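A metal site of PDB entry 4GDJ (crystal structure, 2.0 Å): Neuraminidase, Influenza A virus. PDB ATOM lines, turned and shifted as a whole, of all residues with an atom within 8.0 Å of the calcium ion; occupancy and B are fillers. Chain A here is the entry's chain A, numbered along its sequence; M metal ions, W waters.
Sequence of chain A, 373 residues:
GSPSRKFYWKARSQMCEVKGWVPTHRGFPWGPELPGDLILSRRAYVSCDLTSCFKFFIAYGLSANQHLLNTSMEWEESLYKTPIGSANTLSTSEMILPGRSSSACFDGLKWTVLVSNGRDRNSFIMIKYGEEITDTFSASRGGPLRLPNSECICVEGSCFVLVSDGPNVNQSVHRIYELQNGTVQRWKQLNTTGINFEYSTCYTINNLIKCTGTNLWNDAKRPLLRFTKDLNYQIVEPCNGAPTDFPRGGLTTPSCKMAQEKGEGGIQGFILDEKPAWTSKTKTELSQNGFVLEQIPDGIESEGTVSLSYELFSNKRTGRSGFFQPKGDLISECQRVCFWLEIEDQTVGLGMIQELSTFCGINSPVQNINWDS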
ATOM      1  N   ASN A 196      19.437 -21.576 -13.070  1.00  0.00           N
ATOM      2  CA  ASN A 196      19.770 -22.851 -12.470  1.00  0.00           C
ATOM      3  C   ASN A 196      18.704 -23.815 -12.943  1.00  0.00           C
ATOM      4  O   ASN A 196      17.532 -23.432 -13.073  1.00  0.00           O
ATOM      5  CB  ASN A 196      19.782 -22.692 -10.950  1.00  0.00           C
ATOM      6  CG  ASN A 196      19.843 -23.995 -10.229  1.00  0.00           C
ATOM      7  OD1 ASN A 196      18.883 -24.361  -9.541  1.00  0.00           O
ATOM      8  ND2 ASN A 196      20.955 -24.721 -10.369  1.00  0.00           N
ATOM      9  N   GLY A 213      12.607 -27.681 -15.795  1.00  0.00           N
ATOM     10  CA  GLY A 213      13.607 -27.499 -14.749  1.00  0.00           C
ATOM     11  C   GLY A 213      13.049 -26.821 -13.513  1.00  0.00           C
ATOM     12  O   GLY A 213      11.938 -26.297 -13.505  1.00  0.00           O
ATOM     13  N   THR A 214      13.804 -26.888 -12.449  1.00  0.00           N
ATOM     14  CA  THR A 214      13.494 -26.146 -11.234  1.00  0.00           C
ATOM     15  C   THR A 214      14.679 -25.229 -10.953  1.00  0.00           C
ATOM     16  O   THR A 214      15.841 -25.688 -10.891  1.00  0.00           O
ATOM     17  CB  THR A 214      13.275 -27.096 -10.050  1.00  0.00           C
ATOM     18  OG1 THR A 214      12.196 -27.982 -10.325  1.00  0.00           O
ATOM     19  CG2 THR A 214      13.018 -26.323  -8.735  1.00  0.00           C
ATOM     20  N   ASN A 215      14.409 -23.936 -10.828  1.00  0.00           N
ATOM     21  CA  ASN A 215      15.452 -22.983 -10.564  1.00  0.00           C
ATOM     22  C   ASN A 215      15.508 -22.719  -9.061  1.00  0.00           C
ATOM     23  O   ASN A 215      14.607 -22.120  -8.504  1.00  0.00           O
ATOM     24  CB  ASN A 215      15.247 -21.725 -11.411  1.00  0.00           C
ATOM     25  CG  ASN A 215      16.404 -20.708 -11.268  1.00  0.00           C
ATOM     26  OD1 ASN A 215      17.015 -20.621 -10.228  1.00  0.00           O
ATOM     27  ND2 ASN A 215      16.668 -19.921 -12.311  1.00  0.00           N
ATOM     28  N   LEU A 216      16.549 -23.216  -8.390  1.00  0.00           N
ATOM     29  CA  LEU A 216      16.702 -23.094  -6.954  1.00  0.00           C
ATOM     30  C   LEU A 216      17.418 -21.821  -6.539  1.00  0.00           C
ATOM     31  O   LEU A 216      17.592 -21.540  -5.347  1.00  0.00           O
ATOM     32  CB  LEU A 216      17.483 -24.278  -6.384  1.00  0.00           C
ATOM     33  CG  LEU A 216      16.912 -25.690  -6.592  1.00  0.00           C
ATOM     34  CD1 LEU A 216      17.877 -26.693  -5.990  1.00  0.00           C
ATOM     35  CD2 LEU A 216      15.546 -25.863  -5.947  1.00  0.00           C
ATOM     36  N   TRP A 217      17.801 -21.031  -7.521  1.00  0.00           N
ATOM     37  CA  TRP A 217      18.585 -19.824  -7.244  1.00  0.00           C
ATOM     38  C   TRP A 217      17.753 -18.548  -7.272  1.00  0.00           C
ATOM     39  O   TRP A 217      17.621 -17.861  -6.261  1.00  0.00           O
ATOM     40  CB  TRP A 217      19.703 -19.741  -8.288  1.00  0.00           C
ATOM     41  CG  TRP A 217      20.505 -18.462  -8.343  1.00  0.00           C
ATOM     42  CD1 TRP A 217      20.663 -17.532  -7.354  1.00  0.00           C
ATOM     43  CD2 TRP A 217      21.278 -17.992  -9.465  1.00  0.00           C
ATOM     44  NE1 TRP A 217      21.484 -16.507  -7.787  1.00  0.00           N
ATOM     45  CE2 TRP A 217      21.863 -16.761  -9.079  1.00  0.00           C
ATOM     46  CE3 TRP A 217      21.529 -18.490 -10.748  1.00  0.00           C
ATOM     47  CZ2 TRP A 217      22.679 -16.025  -9.932  1.00  0.00           C
ATOM     48  CZ3 TRP A 217      22.342 -17.767 -11.600  1.00  0.00           C
ATOM     49  CH2 TRP A 217      22.913 -16.544 -11.187  1.00  0.00           C
ATOM     50  N   ASN A 218      17.205 -18.221  -8.439  1.00  0.00           N
ATOM     51  CA  ASN A 218      16.620 -16.900  -8.647  1.00  0.00           C
ATOM     52  C   ASN A 218      15.384 -16.853  -9.543  1.00  0.00           C
ATOM     53  O   ASN A 218      15.209 -15.903 -10.291  1.00  0.00           O
ATOM     54  CB  ASN A 218      17.676 -15.997  -9.272  1.00  0.00           C
ATOM     55  CG  ASN A 218      18.187 -16.523 -10.601  1.00  0.00           C
ATOM     56  OD1 ASN A 218      17.787 -17.603 -11.048  1.00  0.00           O
ATOM     57  ND2 ASN A 218      19.060 -15.763 -11.241  1.00  0.00           N
ATOM     58  N   ASP A 219      14.534 -17.870  -9.495  1.00  0.00           N
ATOM     59  CA  ASP A 219      13.348 -17.876 -10.330  1.00  0.00           C
ATOM     60  C   ASP A 219      12.309 -18.767  -9.686  1.00  0.00           C
ATOM     61  O   ASP A 219      12.629 -19.869  -9.169  1.00  0.00           O
ATOM     62  CB  ASP A 219      13.667 -18.364 -11.735  1.00  0.00           C
ATOM     63  CG  ASP A 219      12.674 -17.894 -12.783  1.00  0.00           C
ATOM     64  OD1 ASP A 219      11.665 -17.217 -12.446  1.00  0.00           O
ATOM     65  OD2 ASP A 219      12.908 -18.248 -13.976  1.00  0.00           O
ATOM     66  N   ALA A 220      11.089 -18.236  -9.684  1.00  0.00           N
ATOM     67  CA  ALA A 220       9.877 -18.938  -9.282  1.00  0.00           C
ATOM     68  C   ALA A 220       9.078 -19.399 -10.497  1.00  0.00           C
ATOM     69  O   ALA A 220       8.134 -20.190 -10.396  1.00  0.00           O
ATOM     70  CB  ALA A 220       9.013 -18.017  -8.414  1.00  0.00           C
ATOM     71  N   LYS A 221       9.451 -18.946 -11.683  1.00  0.00           N
ATOM     72  CA  LYS A 221       8.961 -19.620 -12.875  1.00  0.00           C
ATOM     73  C   LYS A 221       9.883 -20.795 -13.124  1.00  0.00           C
ATOM     74  O   LYS A 221      10.993 -20.808 -12.608  1.00  0.00           O
ATOM     75  CB  LYS A 221       9.027 -18.704 -14.084  1.00  0.00           C
ATOM     76  CG  LYS A 221       7.840 -17.740 -14.257  1.00  0.00           C
ATOM     77  CD  LYS A 221       8.189 -16.634 -15.249  1.00  0.00           C
ATOM     78  CE  LYS A 221       6.910 -15.852 -15.711  1.00  0.00           C
ATOM     79  NZ  LYS A 221       7.303 -14.860 -16.710  1.00  0.00           N
ATOM     80  N   ARG A 222       9.441 -21.767 -13.925  1.00  0.00           N
ATOM     81  CA  ARG A 222      10.303 -22.925 -14.256  1.00  0.00           C
ATOM     82  C   ARG A 222      10.956 -22.788 -15.634  1.00  0.00           C
ATOM     83  O   ARG A 222      10.268 -22.617 -16.644  1.00  0.00           O
ATOM     84  CB  ARG A 222       9.490 -24.232 -14.216  1.00  0.00           C
ATOM     85  CG  ARG A 222       8.863 -24.520 -12.899  1.00  0.00           C
ATOM     86  CD  ARG A 222       8.121 -25.816 -12.864  1.00  0.00           C
ATOM     87  NE  ARG A 222       7.582 -26.090 -11.537  1.00  0.00           N
ATOM     88  CZ  ARG A 222       8.298 -26.554 -10.517  1.00  0.00           C
ATOM     89  NH1 ARG A 222       9.607 -26.803 -10.651  1.00  0.00           N
ATOM     90  NH2 ARG A 222       7.727 -26.788  -9.350  1.00  0.00           N
ATOM     91  N   PRO A 223      12.283 -22.875 -15.698  1.00  0.00           N
ATOM     92  CA  PRO A 223      12.938 -22.880 -17.004  1.00  0.00           C
ATOM     93  C   PRO A 223      12.576 -24.115 -17.794  1.00  0.00           C
ATOM     94  O   PRO A 223      12.335 -25.213 -17.270  1.00  0.00           O
ATOM     95  CB  PRO A 223      14.433 -22.861 -16.634  1.00  0.00           C
ATOM     96  CG  PRO A 223      14.520 -23.394 -15.265  1.00  0.00           C
ATOM     97  CD  PRO A 223      13.261 -22.882 -14.603  1.00  0.00           C
ATOM     98  N   THR A 244       5.113 -21.176 -11.260  1.00  0.00           N
ATOM     99  CA  THR A 244       4.630 -22.448 -10.786  1.00  0.00           C
ATOM    100  C   THR A 244       5.538 -23.218  -9.832  1.00  0.00           C
ATOM    101  O   THR A 244       5.240 -24.359  -9.479  1.00  0.00           O
ATOM    102  CB  THR A 244       4.271 -23.368 -11.949  1.00  0.00           C
ATOM    103  OG1 THR A 244       5.441 -23.696 -12.719  1.00  0.00           O
ATOM    104  CG2 THR A 244       3.228 -22.712 -12.835  1.00  0.00           C
ATOM    105  N   ASP A 245       6.652 -22.630  -9.488  1.00  0.00           N
ATOM    106  CA  ASP A 245       7.547 -23.231  -8.494  1.00  0.00           C
ATOM    107  C   ASP A 245       6.927 -23.061  -7.104  1.00  0.00           C
ATOM    108  O   ASP A 245       5.968 -22.298  -6.910  1.00  0.00           O
ATOM    109  CB  ASP A 245       8.910 -22.545  -8.586  1.00  0.00           C
ATOM    110  CG  ASP A 245      10.076 -23.409  -8.061  1.00  0.00           C
ATOM    111  OD1 ASP A 245       9.856 -24.544  -7.553  1.00  0.00           O
ATOM    112  OD2 ASP A 245      11.217 -22.906  -8.153  1.00  0.00           O
ATOM    113  N   PHE A 246       7.456 -23.794  -6.132  1.00  0.00           N
ATOM    114  CA  PHE A 246       7.169 -23.572  -4.735  1.00  0.00           C
ATOM    115  C   PHE A 246       8.484 -23.598  -3.957  1.00  0.00           C
ATOM    116  O   PHE A 246       9.197 -24.590  -3.991  1.00  0.00           O
ATOM    117  CB  PHE A 246       6.211 -24.623  -4.182  1.00  0.00           C
ATOM    118  CG  PHE A 246       5.614 -24.221  -2.849  1.00  0.00           C
ATOM    119  CD1 PHE A 246       6.356 -24.371  -1.675  1.00  0.00           C
ATOM    120  CD2 PHE A 246       4.356 -23.631  -2.781  1.00  0.00           C
ATOM    121  CE1 PHE A 246       5.830 -23.959  -0.447  1.00  0.00           C
ATOM    122  CE2 PHE A 246       3.814 -23.231  -1.573  1.00  0.00           C
ATOM    123  CZ  PHE A 246       4.552 -23.387  -0.391  1.00  0.00           C
ATOM    124  N   PRO A 247       8.810 -22.521  -3.245  1.00  0.00           N
ATOM    125  CA  PRO A 247       8.029 -21.296  -3.010  1.00  0.00           C
ATOM    126  C   PRO A 247       7.889 -20.378  -4.232  1.00  0.00           C
ATOM    127  O   PRO A 247       8.557 -20.560  -5.230  1.00  0.00           O
ATOM    128  CB  PRO A 247       8.839 -20.583  -1.914  1.00  0.00           C
ATOM    129  CG  PRO A 247      10.241 -21.038  -2.112  1.00  0.00           C
ATOM    130  CD  PRO A 247      10.143 -22.466  -2.591  1.00  0.00           C
ATOM    131  N   ARG A 248       6.992 -19.405  -4.145  1.00  0.00           N
ATOM    132  CA  ARG A 248       6.878 -18.399  -5.179  1.00  0.00           C
ATOM    133  C   ARG A 248       6.153 -17.180  -4.643  1.00  0.00           C
ATOM    134  O   ARG A 248       5.653 -17.179  -3.514  1.00  0.00           O
ATOM    135  CB  ARG A 248       6.125 -18.946  -6.392  1.00  0.00           C
ATOM    136  CG  ARG A 248       4.684 -19.382  -6.091  1.00  0.00           C
ATOM    137  CD  ARG A 248       3.878 -19.700  -7.367  1.00  0.00           C
ATOM    138  NE  ARG A 248       2.499 -20.132  -7.081  1.00  0.00           N
ATOM    139  CZ  ARG A 248       2.140 -21.346  -6.653  1.00  0.00           C
ATOM    140  NH1 ARG A 248       3.030 -22.310  -6.467  1.00  0.00           N
ATOM    141  NH2 ARG A 248       0.852 -21.609  -6.432  1.00  0.00           N
ATOM    142  N   ALA A 259      10.615 -14.628 -12.756  1.00  0.00           N
ATOM    143  CA  ALA A 259       9.896 -14.197 -11.562  1.00  0.00           C
ATOM    144  C   ALA A 259      10.814 -14.311 -10.363  1.00  0.00           C
ATOM    145  O   ALA A 259      10.933 -15.397  -9.760  1.00  0.00           O
ATOM    146  CB  ALA A 259       8.669 -15.029 -11.374  1.00  0.00           C
ATOM    147  N   GLN A 260      11.458 -13.194 -10.018  1.00  0.00           N
ATOM    148  CA  GLN A 260      12.564 -13.230  -9.052  1.00  0.00           C
ATOM    149  C   GLN A 260      12.088 -13.285  -7.625  1.00  0.00           C
ATOM    150  O   GLN A 260      12.816 -13.732  -6.726  1.00  0.00           O
ATOM    151  CB  GLN A 260      13.489 -12.032  -9.250  1.00  0.00           C
ATOM    152  CG  GLN A 260      14.081 -11.969 -10.656  1.00  0.00           C
ATOM    153  CD  GLN A 260      15.603 -12.046 -10.674  1.00  0.00           C
ATOM    154  OE1 GLN A 260      16.277 -11.236 -10.029  1.00  0.00           O
ATOM    155  NE2 GLN A 260      16.146 -13.025 -11.405  1.00  0.00           N
ATOM    156  N   GLU A 261      10.849 -12.878  -7.392  1.00  0.00           N
ATOM    157  CA  GLU A 261      10.340 -12.858  -6.054  1.00  0.00           C
ATOM    158  C   GLU A 261      10.169 -14.282  -5.504  1.00  0.00           C
ATOM    159  O   GLU A 261       9.472 -15.117  -6.085  1.00  0.00           O
ATOM    160  CB  GLU A 261       8.993 -12.114  -6.003  1.00  0.00           C
ATOM    161  CG  GLU A 261       8.453 -12.015  -4.607  1.00  0.00           C
ATOM    162  CD  GLU A 261       7.099 -11.311  -4.536  1.00  0.00           C
ATOM    163  OE1 GLU A 261       6.524 -10.970  -5.610  1.00  0.00           O
ATOM    164  OE2 GLU A 261       6.618 -11.116  -3.397  1.00  0.00           O
ATOM    165  N   LYS A 262      10.792 -14.521  -4.361  1.00  0.00           N
ATOM    166  CA  LYS A 262      10.831 -15.833  -3.748  1.00  0.00           C
ATOM    167  C   LYS A 262      11.345 -16.864  -4.766  1.00  0.00           C
ATOM    168  O   LYS A 262      10.892 -17.995  -4.816  1.00  0.00           O
ATOM    169  CB  LYS A 262       9.453 -16.176  -3.162  1.00  0.00           C
ATOM    170  CG  LYS A 262       9.261 -15.391  -1.838  1.00  0.00           C
ATOM    171  CD  LYS A 262       7.856 -15.417  -1.329  1.00  0.00           C
ATOM    172  CE  LYS A 262       7.521 -16.708  -0.591  1.00  0.00           C
ATOM    173  NZ  LYS A 262       6.030 -16.924  -0.544  1.00  0.00           N
ATOM    174  N   GLY A 263      12.288 -16.438  -5.588  1.00  0.00           N
ATOM    175  CA  GLY A 263      12.870 -17.309  -6.578  1.00  0.00           C
ATOM    176  C   GLY A 263      13.797 -18.352  -5.961  1.00  0.00           C
ATOM    177  O   GLY A 263      13.954 -19.442  -6.508  1.00  0.00           O
ATOM    178  N   GLU A 264      14.419 -18.013  -4.840  1.00  0.00           N
ATOM    179  CA  GLU A 264      15.348 -18.959  -4.201  1.00  0.00           C
ATOM    180  C   GLU A 264      14.585 -20.167  -3.666  1.00  0.00           C
ATOM    181  O   GLU A 264      13.482 -20.023  -3.144  1.00  0.00           O
ATOM    182  CB  GLU A 264      16.112 -18.259  -3.059  1.00  0.00           C
ATOM    183  CG  GLU A 264      17.148 -19.132  -2.422  1.00  0.00           C
ATOM    184  CD  GLU A 264      17.961 -18.404  -1.327  1.00  0.00           C
ATOM    185  OE1 GLU A 264      17.660 -17.229  -1.016  1.00  0.00           O
ATOM    186  OE2 GLU A 264      18.881 -19.025  -0.776  1.00  0.00           O
ATOM    187  N   GLY A 265      15.187 -21.349  -3.778  1.00  0.00           N
ATOM    188  CA  GLY A 265      14.538 -22.582  -3.362  1.00  0.00           C
ATOM    189  C   GLY A 265      13.619 -23.107  -4.490  1.00  0.00           C
ATOM    190  O   GLY A 265      13.530 -22.514  -5.570  1.00  0.00           O
ATOM    191  N   GLY A 266      12.936 -24.212  -4.235  1.00  0.00           N
ATOM    192  CA  GLY A 266      12.110 -24.771  -5.289  1.00  0.00           C
ATOM    193  C   GLY A 266      11.834 -26.229  -5.076  1.00  0.00           C
ATOM    194  O   GLY A 266      12.375 -26.852  -4.150  1.00  0.00           O
ATOM    195  N   ILE A 267      10.940 -26.768  -5.914  1.00  0.00           N
ATOM    196  CA  ILE A 267      10.594 -28.175  -5.846  1.00  0.00           C
ATOM    197  C   ILE A 267      10.373 -28.703  -7.267  1.00  0.00           C
ATOM    198  O   ILE A 267       9.959 -27.973  -8.170  1.00  0.00           O
ATOM    199  CB  ILE A 267       9.348 -28.390  -4.961  1.00  0.00           C
ATOM    200  CG1 ILE A 267       9.091 -29.882  -4.734  1.00  0.00           C
ATOM    201  CG2 ILE A 267       8.135 -27.738  -5.542  1.00  0.00           C
ATOM    202  CD1 ILE A 267       8.176 -30.159  -3.519  1.00  0.00           C
HETATM  203 CA    CA M   1      12.799 -21.316  -7.381  1.00  0.00          CA
HETATM  204  O   HOH W   1      11.090 -20.290  -6.090  1.00  0.00           O
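Within 4 Å of the calcium ion: Asn 215, Asp 219, Asp 245, Gly 263 and Gly 265. Along chain A the residues within 4 Å of the calcium ion span positions 215 to 265. The nearest printed residue that does not touch the calcium ion is Gly 266 (4.1 Å).
The calcium ion is bound by the backbone carbonyl oxygen (O) of Asn 215, at 2.3 Å. The backbone carbonyl oxygen (O) of Gly 265 binds the calcium ion (2.3 Å). O of Asp 219 is bound to the calcium ion (2.3 Å). The calcium ion is bound by the backbone carbonyl oxygen (O) of Gly 263 (2.4 Å). OD2 of Asp 245 is bound to the calcium ion. Water W1 is bound to the calcium ion (2.4 Å). The calcium ion has six donor atoms within binding distance.
N of Trp 217 is in hydrogen-bond range of OD1 of Asn 215, 2.8 Å away. The side-chain amide nitrogen of Asn 215 is in hydrogen-bond range of the side-chain amide oxygen of Asn 218. The side-chain amide nitrogen (ND2) of Asn 215 sits close to the backbone NH (N) of Asn 196 (3.3 Å). The backbone NH (N) of Gly 265 sits at hydrogen-bond distance from the backbone carbonyl oxygen (O) of Leu 216, 2.9 Å away. N of Lys 221 lies within hydrogen-bond range of OD1 of Asp 219, 2.9 Å away. OD1 of Asp 219 is in hydrogen-bond range of N of Ala 259 (2.8 Å). The backbone NH (N) of Asp 245 lies within hydrogen-bond range of the backbone carbonyl oxygen (O) of Ala 220 (3.0 Å). NH2 of Arg 222 is in salt-bridge range of OD1 of Asp 245 (3.6 Å).
Water W1 bridges the backbone carbonyl oxygen (O) of Lys 262 (2.6 Å) and the backbone carbonyl oxygen (O) of Pro 247 (2.7 Å).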
